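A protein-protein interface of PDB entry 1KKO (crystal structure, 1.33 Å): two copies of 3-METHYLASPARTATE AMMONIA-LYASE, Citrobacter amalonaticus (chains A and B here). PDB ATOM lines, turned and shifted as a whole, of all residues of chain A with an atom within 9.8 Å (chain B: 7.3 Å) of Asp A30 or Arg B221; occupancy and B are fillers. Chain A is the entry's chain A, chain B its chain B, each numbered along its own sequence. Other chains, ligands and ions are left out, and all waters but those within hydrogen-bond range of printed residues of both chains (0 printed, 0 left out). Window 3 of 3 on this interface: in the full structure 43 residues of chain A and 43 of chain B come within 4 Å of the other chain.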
ATOM      1  N   ALA A  27      -1.410  18.587  -4.635  1.00  0.00           N
ATOM      2  CA  ALA A  27      -1.484  19.031  -6.028  1.00  0.00           C
ATOM      3  C   ALA A  27      -2.512  20.122  -6.185  1.00  0.00           C
ATOM      4  O   ALA A  27      -3.641  20.011  -5.714  1.00  0.00           O
ATOM      5  CB  ALA A  27      -1.803  17.874  -6.959  1.00  0.00           C
ATOM      6  N   GLY A  28      -2.105  21.194  -6.848  1.00  0.00           N
ATOM      7  CA  GLY A  28      -3.011  22.278  -7.120  1.00  0.00           C
ATOM      8  C   GLY A  28      -3.866  21.871  -8.299  1.00  0.00           C
ATOM      9  O   GLY A  28      -3.744  20.768  -8.849  1.00  0.00           O
ATOM     10  N   HIS A  29      -4.743  22.764  -8.698  1.00  0.00           N
ATOM     11  CA  HIS A  29      -5.572  22.463  -9.834  1.00  0.00           C
ATOM     12  C   HIS A  29      -5.839  23.698 -10.650  1.00  0.00           C
ATOM     13  O   HIS A  29      -5.673  24.839 -10.200  1.00  0.00           O
ATOM     14  CB  HIS A  29      -6.880  21.833  -9.388  1.00  0.00           C
ATOM     15  CG  HIS A  29      -7.765  22.769  -8.644  1.00  0.00           C
ATOM     16  ND1 HIS A  29      -7.655  22.973  -7.285  1.00  0.00           N
ATOM     17  CD2 HIS A  29      -8.768  23.570  -9.069  1.00  0.00           C
ATOM     18  CE1 HIS A  29      -8.556  23.863  -6.906  1.00  0.00           C
ATOM     19  NE2 HIS A  29      -9.246  24.238  -7.969  1.00  0.00           N
ATOM     20  N   ASP A  30      -6.237  23.428 -11.880  1.00  0.00           N
ATOM     21  CA  ASP A  30      -6.605  24.442 -12.837  1.00  0.00           C
ATOM     22  C   ASP A  30      -7.844  23.852 -13.477  1.00  0.00           C
ATOM     23  O   ASP A  30      -7.753  22.922 -14.289  1.00  0.00           O
ATOM     24  CB  ASP A  30      -5.500  24.639 -13.860  1.00  0.00           C
ATOM     25  CG  ASP A  30      -5.774  25.795 -14.803  1.00  0.00           C
ATOM     26  OD1 ASP A  30      -6.930  25.967 -15.230  1.00  0.00           O
ATOM     27  OD2 ASP A  30      -4.878  26.602 -15.158  1.00  0.00           O
ATOM     28  N   GLY A  31      -8.994  24.369 -13.091  1.00  0.00           N
ATOM     29  CA  GLY A  31     -10.250  23.790 -13.520  1.00  0.00           C
ATOM     30  C   GLY A  31     -10.338  22.363 -13.001  1.00  0.00           C
ATOM     31  O   GLY A  31     -10.165  22.117 -11.808  1.00  0.00           O
ATOM     32  N   PHE A  32     -10.584  21.419 -13.904  1.00  0.00           N
ATOM     33  CA  PHE A  32     -10.685  20.004 -13.542  1.00  0.00           C
ATOM     34  C   PHE A  32      -9.339  19.301 -13.522  1.00  0.00           C
ATOM     35  O   PHE A  32      -9.250  18.137 -13.126  1.00  0.00           O
ATOM     36  CB  PHE A  32     -11.561  19.316 -14.585  1.00  0.00           C
ATOM     37  CG  PHE A  32     -12.124  17.985 -14.164  1.00  0.00           C
ATOM     38  CD1 PHE A  32     -13.062  17.896 -13.152  1.00  0.00           C
ATOM     39  CD2 PHE A  32     -11.754  16.825 -14.817  1.00  0.00           C
ATOM     40  CE1 PHE A  32     -13.597  16.677 -12.795  1.00  0.00           C
ATOM     41  CE2 PHE A  32     -12.299  15.610 -14.462  1.00  0.00           C
ATOM     42  CZ  PHE A  32     -13.211  15.541 -13.443  1.00  0.00           C
ATOM     43  N   ILE A  33      -8.293  19.998 -13.942  1.00  0.00           N
ATOM     44  CA  ILE A  33      -6.982  19.411 -14.129  1.00  0.00           C
ATOM     45  C   ILE A  33      -6.110  19.607 -12.898  1.00  0.00           C
ATOM     46  O   ILE A  33      -5.961  20.723 -12.427  1.00  0.00           O
ATOM     47  CB  ILE A  33      -6.287  20.073 -15.371  1.00  0.00           C
ATOM     48  CG1 ILE A  33      -7.207  20.046 -16.593  1.00  0.00           C
ATOM     49  CG2 ILE A  33      -4.952  19.406 -15.662  1.00  0.00           C
ATOM     50  CD1 ILE A  33      -7.692  18.672 -16.959  1.00  0.00           C
ATOM     51  N   TYR A  34      -5.532  18.534 -12.385  1.00  0.00           N
ATOM     52  CA  TYR A  34      -4.561  18.660 -11.297  1.00  0.00           C
ATOM     53  C   TYR A  34      -3.206  18.985 -11.882  1.00  0.00           C
ATOM     54  O   TYR A  34      -2.809  18.414 -12.902  1.00  0.00           O
ATOM     55  CB  TYR A  34      -4.490  17.373 -10.480  1.00  0.00           C
ATOM     56  CG  TYR A  34      -5.583  17.269  -9.451  1.00  0.00           C
ATOM     57  CD1 TYR A  34      -5.557  18.048  -8.306  1.00  0.00           C
ATOM     58  CD2 TYR A  34      -6.652  16.403  -9.616  1.00  0.00           C
ATOM     59  CE1 TYR A  34      -6.549  17.967  -7.358  1.00  0.00           C
ATOM     60  CE2 TYR A  34      -7.656  16.318  -8.658  1.00  0.00           C
ATOM     61  CZ  TYR A  34      -7.595  17.102  -7.532  1.00  0.00           C
ATOM     62  OH  TYR A  34      -8.579  17.048  -6.568  1.00  0.00           O
ATOM     63  N   THR A  35      -2.488  19.897 -11.230  1.00  0.00           N
ATOM     64  CA  THR A  35      -1.181  20.320 -11.711  1.00  0.00           C
ATOM     65  C   THR A  35      -0.041  19.581 -11.027  1.00  0.00           C
ATOM     66  O   THR A  35      -0.255  18.802 -10.102  1.00  0.00           O
ATOM     67  CB  THR A  35      -0.994  21.824 -11.519  1.00  0.00           C
ATOM     68  OG1 THR A  35      -1.123  22.155 -10.136  1.00  0.00           O
ATOM     69  CG2 THR A  35      -2.100  22.608 -12.221  1.00  0.00           C
ATOM     70  N   GLY A  36       1.173  19.856 -11.488  1.00  0.00           N
ATOM     71  CA  GLY A  36       2.344  19.169 -10.985  1.00  0.00           C
ATOM     72  C   GLY A  36       2.481  17.804 -11.629  1.00  0.00           C
ATOM     73  O   GLY A  36       1.705  17.424 -12.522  1.00  0.00           O
ATOM     74  N   VAL A  46      -1.599  13.578 -13.133  1.00  0.00           N
ATOM     75  CA  VAL A  46      -2.247  13.360 -11.848  1.00  0.00           C
ATOM     76  C   VAL A  46      -3.676  12.834 -12.057  1.00  0.00           C
ATOM     77  O   VAL A  46      -4.151  11.992 -11.286  1.00  0.00           O
ATOM     78  CB  VAL A  46      -2.227  14.627 -10.964  1.00  0.00           C
ATOM     79  CG1 VAL A  46      -3.026  14.413  -9.707  1.00  0.00           C
ATOM     80  CG2 VAL A  46      -0.782  14.970 -10.586  1.00  0.00           C
ATOM     81  N   ARG A  47      -4.341  13.330 -13.094  1.00  0.00           N
ATOM     82  CA  ARG A  47      -5.673  12.881 -13.445  1.00  0.00           C
ATOM     83  C   ARG A  47      -5.676  12.482 -14.914  1.00  0.00           C
ATOM     84  O   ARG A  47      -5.210  13.238 -15.765  1.00  0.00           O
ATOM     85  CB  ARG A  47      -6.690  13.988 -13.169  1.00  0.00           C
ATOM     86  CG  ARG A  47      -8.046  13.790 -13.760  1.00  0.00           C
ATOM     87  CD  ARG A  47      -9.062  14.730 -13.192  1.00  0.00           C
ATOM     88  NE  ARG A  47      -9.482  14.295 -11.873  1.00  0.00           N
ATOM     89  CZ  ARG A  47     -10.227  15.001 -11.051  1.00  0.00           C
ATOM     90  NH1 ARG A  47     -10.611  14.474  -9.903  1.00  0.00           N
ATOM     91  NH2 ARG A  47     -10.569  16.251 -11.354  1.00  0.00           N
ATOM     92  N   TYR B 178     -17.317  25.261 -17.637  1.00  0.00           N
ATOM     93  CA  TYR B 178     -15.867  25.371 -17.623  1.00  0.00           C
ATOM     94  C   TYR B 178     -15.263  24.013 -17.288  1.00  0.00           C
ATOM     95  O   TYR B 178     -14.470  23.482 -18.050  1.00  0.00           O
ATOM     96  CB  TYR B 178     -15.380  26.473 -16.665  1.00  0.00           C
ATOM     97  CG  TYR B 178     -15.949  27.811 -17.046  1.00  0.00           C
ATOM     98  CD1 TYR B 178     -15.444  28.518 -18.122  1.00  0.00           C
ATOM     99  CD2 TYR B 178     -17.029  28.352 -16.366  1.00  0.00           C
ATOM    100  CE1 TYR B 178     -15.967  29.735 -18.488  1.00  0.00           C
ATOM    101  CE2 TYR B 178     -17.561  29.566 -16.729  1.00  0.00           C
ATOM    102  CZ  TYR B 178     -17.027  30.258 -17.791  1.00  0.00           C
ATOM    103  OH  TYR B 178     -17.557  31.480 -18.169  1.00  0.00           O
ATOM    104  N   ILE B 179     -15.681  23.441 -16.163  1.00  0.00           N
ATOM    105  CA  ILE B 179     -15.158  22.157 -15.724  1.00  0.00           C
ATOM    106  C   ILE B 179     -15.463  21.044 -16.724  1.00  0.00           C
ATOM    107  O   ILE B 179     -14.609  20.220 -17.025  1.00  0.00           O
ATOM    108  CB  ILE B 179     -15.719  21.824 -14.318  1.00  0.00           C
ATOM    109  CG1 ILE B 179     -15.170  22.810 -13.278  1.00  0.00           C
ATOM    110  CG2 ILE B 179     -15.452  20.370 -13.967  1.00  0.00           C
ATOM    111  CD1 ILE B 179     -13.699  22.785 -13.110  1.00  0.00           C
ATOM    112  N   VAL B 181     -15.842  21.190 -19.856  1.00  0.00           N
ATOM    113  CA  VAL B 181     -15.013  21.301 -21.036  1.00  0.00           C
ATOM    114  C   VAL B 181     -13.711  20.537 -20.830  1.00  0.00           C
ATOM    115  O   VAL B 181     -13.249  19.846 -21.737  1.00  0.00           O
ATOM    116  CB  VAL B 181     -14.760  22.780 -21.383  1.00  0.00           C
ATOM    117  CG1 VAL B 181     -13.586  22.947 -22.320  1.00  0.00           C
ATOM    118  CG2 VAL B 181     -16.019  23.372 -22.000  1.00  0.00           C
ATOM    119  N   ASP B 182     -13.108  20.653 -19.650  1.00  0.00           N
ATOM    120  CA  ASP B 182     -11.878  19.914 -19.383  1.00  0.00           C
ATOM    121  C   ASP B 182     -12.116  18.406 -19.466  1.00  0.00           C
ATOM    122  O   ASP B 182     -11.291  17.680 -20.008  1.00  0.00           O
ATOM    123  CB  ASP B 182     -11.319  20.235 -18.001  1.00  0.00           C
ATOM    124  CG  ASP B 182     -10.846  21.647 -17.856  1.00  0.00           C
ATOM    125  OD1 ASP B 182     -10.727  22.355 -18.883  1.00  0.00           O
ATOM    126  OD2 ASP B 182     -10.559  22.112 -16.719  1.00  0.00           O
ATOM    127  N   ILE B 185     -12.326  17.463 -23.151  1.00  0.00           N
ATOM    128  CA  ILE B 185     -11.036  17.467 -23.824  1.00  0.00           C
ATOM    129  C   ILE B 185     -10.269  16.193 -23.430  1.00  0.00           C
ATOM    130  O   ILE B 185      -9.689  15.514 -24.272  1.00  0.00           O
ATOM    131  CB  ILE B 185     -10.238  18.716 -23.438  1.00  0.00           C
ATOM    132  CG1 ILE B 185     -10.914  19.976 -23.978  1.00  0.00           C
ATOM    133  CG2 ILE B 185      -8.806  18.629 -23.953  1.00  0.00           C
ATOM    134  CD1 ILE B 185     -10.450  21.229 -23.291  1.00  0.00           C
ATOM    135  N   VAL B 215     -16.593  31.829 -25.936  1.00  0.00           N
ATOM    136  CA  VAL B 215     -16.099  31.096 -27.098  1.00  0.00           C
ATOM    137  C   VAL B 215     -14.580  31.170 -27.154  1.00  0.00           C
ATOM    138  O   VAL B 215     -13.915  30.186 -27.453  1.00  0.00           O
ATOM    139  CB  VAL B 215     -16.734  31.593 -28.410  1.00  0.00           C
ATOM    140  CG1 VAL B 215     -16.124  30.869 -29.606  1.00  0.00           C
ATOM    141  CG2 VAL B 215     -18.228  31.384 -28.366  1.00  0.00           C
ATOM    142  N   ARG B 216     -14.021  32.344 -26.880  1.00  0.00           N
ATOM    143  CA  ARG B 216     -12.581  32.502 -26.848  1.00  0.00           C
ATOM    144  C   ARG B 216     -11.952  31.668 -25.724  1.00  0.00           C
ATOM    145  O   ARG B 216     -10.926  31.033 -25.927  1.00  0.00           O
ATOM    146  CB  ARG B 216     -12.202  33.983 -26.716  1.00  0.00           C
ATOM    147  CG  ARG B 216     -10.707  34.248 -26.571  1.00  0.00           C
ATOM    148  CD  ARG B 216      -9.870  33.792 -27.715  1.00  0.00           C
ATOM    149  NE  ARG B 216     -10.209  34.533 -28.919  1.00  0.00           N
ATOM    150  CZ  ARG B 216      -9.341  34.878 -29.859  1.00  0.00           C
ATOM    151  NH1 ARG B 216      -8.065  34.539 -29.748  1.00  0.00           N
ATOM    152  NH2 ARG B 216      -9.760  35.549 -30.920  1.00  0.00           N
ATOM    153  N   TRP B 217     -12.568  31.665 -24.548  1.00  0.00           N
ATOM    154  CA  TRP B 217     -12.081  30.856 -23.441  1.00  0.00           C
ATOM    155  C   TRP B 217     -12.056  29.371 -23.838  1.00  0.00           C
ATOM    156  O   TRP B 217     -11.093  28.648 -23.589  1.00  0.00           O
ATOM    157  CB  TRP B 217     -12.950  31.043 -22.177  1.00  0.00           C
ATOM    158  CG  TRP B 217     -12.464  30.175 -21.064  1.00  0.00           C
ATOM    159  CD1 TRP B 217     -11.519  30.484 -20.135  1.00  0.00           C
ATOM    160  CD2 TRP B 217     -12.848  28.825 -20.810  1.00  0.00           C
ATOM    161  NE1 TRP B 217     -11.299  29.406 -19.312  1.00  0.00           N
ATOM    162  CE2 TRP B 217     -12.103  28.375 -19.712  1.00  0.00           C
ATOM    163  CE3 TRP B 217     -13.764  27.946 -21.399  1.00  0.00           C
ATOM    164  CZ2 TRP B 217     -12.236  27.086 -19.200  1.00  0.00           C
ATOM    165  CZ3 TRP B 217     -13.884  26.661 -20.888  1.00  0.00           C
ATOM    166  CH2 TRP B 217     -13.125  26.249 -19.815  1.00  0.00           C
ATOM    167  N   LEU B 218     -13.147  28.950 -24.458  1.00  0.00           N
ATOM    168  CA  LEU B 218     -13.358  27.578 -24.883  1.00  0.00           C
ATOM    169  C   LEU B 218     -12.325  27.127 -25.915  1.00  0.00           C
ATOM    170  O   LEU B 218     -11.695  26.083 -25.757  1.00  0.00           O
ATOM    171  CB  LEU B 218     -14.764  27.473 -25.455  1.00  0.00           C
ATOM    172  CG  LEU B 218     -15.162  26.171 -26.127  1.00  0.00           C
ATOM    173  CD1 LEU B 218     -15.050  24.965 -25.196  1.00  0.00           C
ATOM    174  CD2 LEU B 218     -16.571  26.322 -26.657  1.00  0.00           C
ATOM    175  N   SER B 219     -12.141  27.895 -26.980  1.00  0.00           N
ATOM    176  CA  SER B 219     -11.147  27.507 -27.974  1.00  0.00           C
ATOM    177  C   SER B 219      -9.746  27.580 -27.387  1.00  0.00           C
ATOM    178  O   SER B 219      -8.930  26.713 -27.651  1.00  0.00           O
ATOM    179  CB  SER B 219     -11.291  28.325 -29.247  1.00  0.00           C
ATOM    180  OG  SER B 219     -11.079  29.698 -29.009  1.00  0.00           O
ATOM    181  N   ASP B 220      -9.460  28.586 -26.572  1.00  0.00           N
ATOM    182  CA  ASP B 220      -8.162  28.649 -25.922  1.00  0.00           C
ATOM    183  C   ASP B 220      -7.941  27.399 -25.058  1.00  0.00           C
ATOM    184  O   ASP B 220      -6.852  26.849 -25.042  1.00  0.00           O
ATOM    185  CB  ASP B 220      -8.053  29.862 -24.991  1.00  0.00           C
ATOM    186  CG  ASP B 220      -7.616  31.132 -25.683  1.00  0.00           C
ATOM    187  OD1 ASP B 220      -7.044  31.075 -26.795  1.00  0.00           O
ATOM    188  OD2 ASP B 220      -7.810  32.237 -25.124  1.00  0.00           O
ATOM    189  N   ARG B 221      -8.970  26.972 -24.330  1.00  0.00           N
ATOM    190  CA  ARG B 221      -8.849  25.838 -23.420  1.00  0.00           C
ATOM    191  C   ARG B 221      -8.555  24.557 -24.194  1.00  0.00           C
ATOM    192  O   ARG B 221      -7.692  23.766 -23.815  1.00  0.00           O
ATOM    193  CB  ARG B 221     -10.122  25.683 -22.583  1.00  0.00           C
ATOM    194  CG  ARG B 221      -9.966  24.773 -21.377  1.00  0.00           C
ATOM    195  CD  ARG B 221      -9.154  25.408 -20.272  1.00  0.00           C
ATOM    196  NE  ARG B 221      -9.138  24.581 -19.080  1.00  0.00           N
ATOM    197  CZ  ARG B 221      -8.375  24.822 -18.028  1.00  0.00           C
ATOM    198  NH1 ARG B 221      -7.579  25.885 -17.985  1.00  0.00           N
ATOM    199  NH2 ARG B 221      -8.423  23.995 -16.999  1.00  0.00           N
ATOM    200  N   ILE B 222      -9.285  24.346 -25.273  1.00  0.00           N
ATOM    201  CA  ILE B 222      -9.067  23.172 -26.103  1.00  0.00           C
ATOM    202  C   ILE B 222      -7.638  23.162 -26.643  1.00  0.00           C
ATOM    203  O   ILE B 222      -6.925  22.159 -26.570  1.00  0.00           O
ATOM    204  CB  ILE B 222     -10.096  23.159 -27.245  1.00  0.00           C
ATOM    205  CG1 ILE B 222     -11.491  22.900 -26.671  1.00  0.00           C
ATOM    206  CG2 ILE B 222      -9.717  22.130 -28.310  1.00  0.00           C
ATOM    207  CD1 ILE B 222     -12.581  23.236 -27.616  1.00  0.00           C
ATOM    208  N   LEU B 223      -7.221  24.296 -27.197  1.00  0.00           N
ATOM    209  CA  LEU B 223      -5.895  24.401 -27.792  1.00  0.00           C
ATOM    210  C   LEU B 223      -4.791  24.233 -26.752  1.00  0.00           C
ATOM    211  O   LEU B 223      -3.722  23.710 -27.073  1.00  0.00           O
ATOM    212  CB  LEU B 223      -5.756  25.733 -28.541  1.00  0.00           C
ATOM    213  CG  LEU B 223      -6.300  25.781 -29.973  1.00  0.00           C
ATOM    214  CD1 LEU B 223      -7.560  24.991 -30.158  1.00  0.00           C
ATOM    215  CD2 LEU B 223      -6.530  27.220 -30.429  1.00  0.00           C
ATOM    216  N   SER B 224      -5.035  24.638 -25.510  1.00  0.00           N
ATOM    217  CA  SER B 224      -4.031  24.537 -24.451  1.00  0.00           C
ATOM    218  C   SER B 224      -3.954  23.150 -23.818  1.00  0.00           C
ATOM    219  O   SER B 224      -2.864  22.608 -23.608  1.00  0.00           O
ATOM    220  CB  SER B 224      -4.329  25.565 -23.357  1.00  0.00           C
ATOM    221  OG  SER B 224      -3.515  25.357 -22.211  1.00  0.00           O
ATOM    222  N   LEU B 225      -5.101  22.566 -23.513  1.00  0.00           N
ATOM    223  CA  LEU B 225      -5.149  21.300 -22.791  1.00  0.00           C
ATOM    224  C   LEU B 225      -4.949  20.068 -23.664  1.00  0.00           C
ATOM    225  O   LEU B 225      -4.503  19.030 -23.183  1.00  0.00           O
ATOM    226  CB  LEU B 225      -6.485  21.169 -22.041  1.00  0.00           C
ATOM    227  CG  LEU B 225      -6.509  21.552 -20.566  1.00  0.00           C
ATOM    228  CD1 LEU B 225      -5.476  20.693 -19.847  1.00  0.00           C
ATOM    229  CD2 LEU B 225      -6.270  23.033 -20.401  1.00  0.00           C
ATOM    230  N   ARG B 226      -5.307  20.147 -24.935  1.00  0.00           N
ATOM    231  CA  ARG B 226      -5.190  18.970 -25.788  1.00  0.00           C
ATOM    232  C   ARG B 226      -3.753  18.472 -25.843  1.00  0.00           C
ATOM    233  O   ARG B 226      -2.805  19.243 -25.749  1.00  0.00           O
ATOM    234  CB  ARG B 226      -5.722  19.246 -27.194  1.00  0.00           C
ATOM    235  CG  ARG B 226      -4.862  20.169 -28.001  1.00  0.00           C
ATOM    236  CD  ARG B 226      -5.464  20.512 -29.348  1.00  0.00           C
ATOM    237  NE  ARG B 226      -4.631  21.451 -30.080  1.00  0.00           N
ATOM    238  CZ  ARG B 226      -4.959  21.991 -31.239  1.00  0.00           C
ATOM    239  NH1 ARG B 226      -6.091  21.653 -31.827  1.00  0.00           N
ATOM    240  NH2 ARG B 226      -4.140  22.852 -31.826  1.00  0.00           N
ATOM    241  N   GLN B 266     -11.147  30.276 -33.292  1.00  0.00           N
ATOM    242  CA  GLN B 266      -9.779  29.906 -33.644  1.00  0.00           C
ATOM    243  C   GLN B 266      -9.663  28.670 -34.522  1.00  0.00           C
ATOM    244  O   GLN B 266      -8.841  27.799 -34.278  1.00  0.00           O
ATOM    245  CB  GLN B 266      -8.947  29.738 -32.381  1.00  0.00           C
ATOM    246  CG  GLN B 266      -8.874  30.994 -31.540  1.00  0.00           C
ATOM    247  CD  GLN B 266      -7.873  30.882 -30.408  1.00  0.00           C
ATOM    248  OE1 GLN B 266      -6.678  31.141 -30.598  1.00  0.00           O
ATOM    249  NE2 GLN B 266      -8.350  30.512 -29.227  1.00  0.00           N
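NH1 of Arg B221 lies within salt-bridge range of OD1 of Asp A30 (2.8 Å).
The backbone NH (N) of Phe A32 sits at hydrogen-bond distance from the side-chain carboxylate (OD2) of Asp B182 (2.9 Å).
The guanidinium group of Arg A47 sits at hydrogen-bond distance from the backbone carbonyl oxygen of Phe A32, 2.9 Å away.
The guanidinium group (NE) of Arg B221 is in salt-bridge range of the side-chain carboxylate (OD1) of Asp B182 (2.7 Å).
Among the printed residues, pairs that only touch across the chains: Gly A31 with Ile B179, Phe A32 with Ile B179, Gly A31 with Asp B182, Ile A33 with Leu B225, Asp A30 with Asp B182, Gly A31 with Arg B221 and Ile A33 with Asp B182.
Asp A30 touches two residues of chain B.
Of the printed residues of chain B, Gly A31 touches Ile B179 (3.4 Å), Asp B182 (3.6 Å) and Arg B221 (3.9 Å).
Val A46 touches none of the printed residues of chain B.
Of the printed residues of chain A, Ile B179 touches Gly A31 and Phe A32.
Of the printed residues of chain A, Asp B182 touches Asp A30, Gly A31, Phe A32 and Ile A33.
No residue of chain A comes within 4 Å of Asp B220.
No residue of chain A comes within 4 Å of Ile B222.
Leu B223 touches none of the printed residues of chain A.
Ser B224 touches none of the printed residues of chain A.
The nearest printed residue of chain B that does not touch Asp A30 is Ile B179 (6.0 Å).
Of the 18 printed residues of chain B, 4 touch a printed residue of chain A.
No position is printed for both chains.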
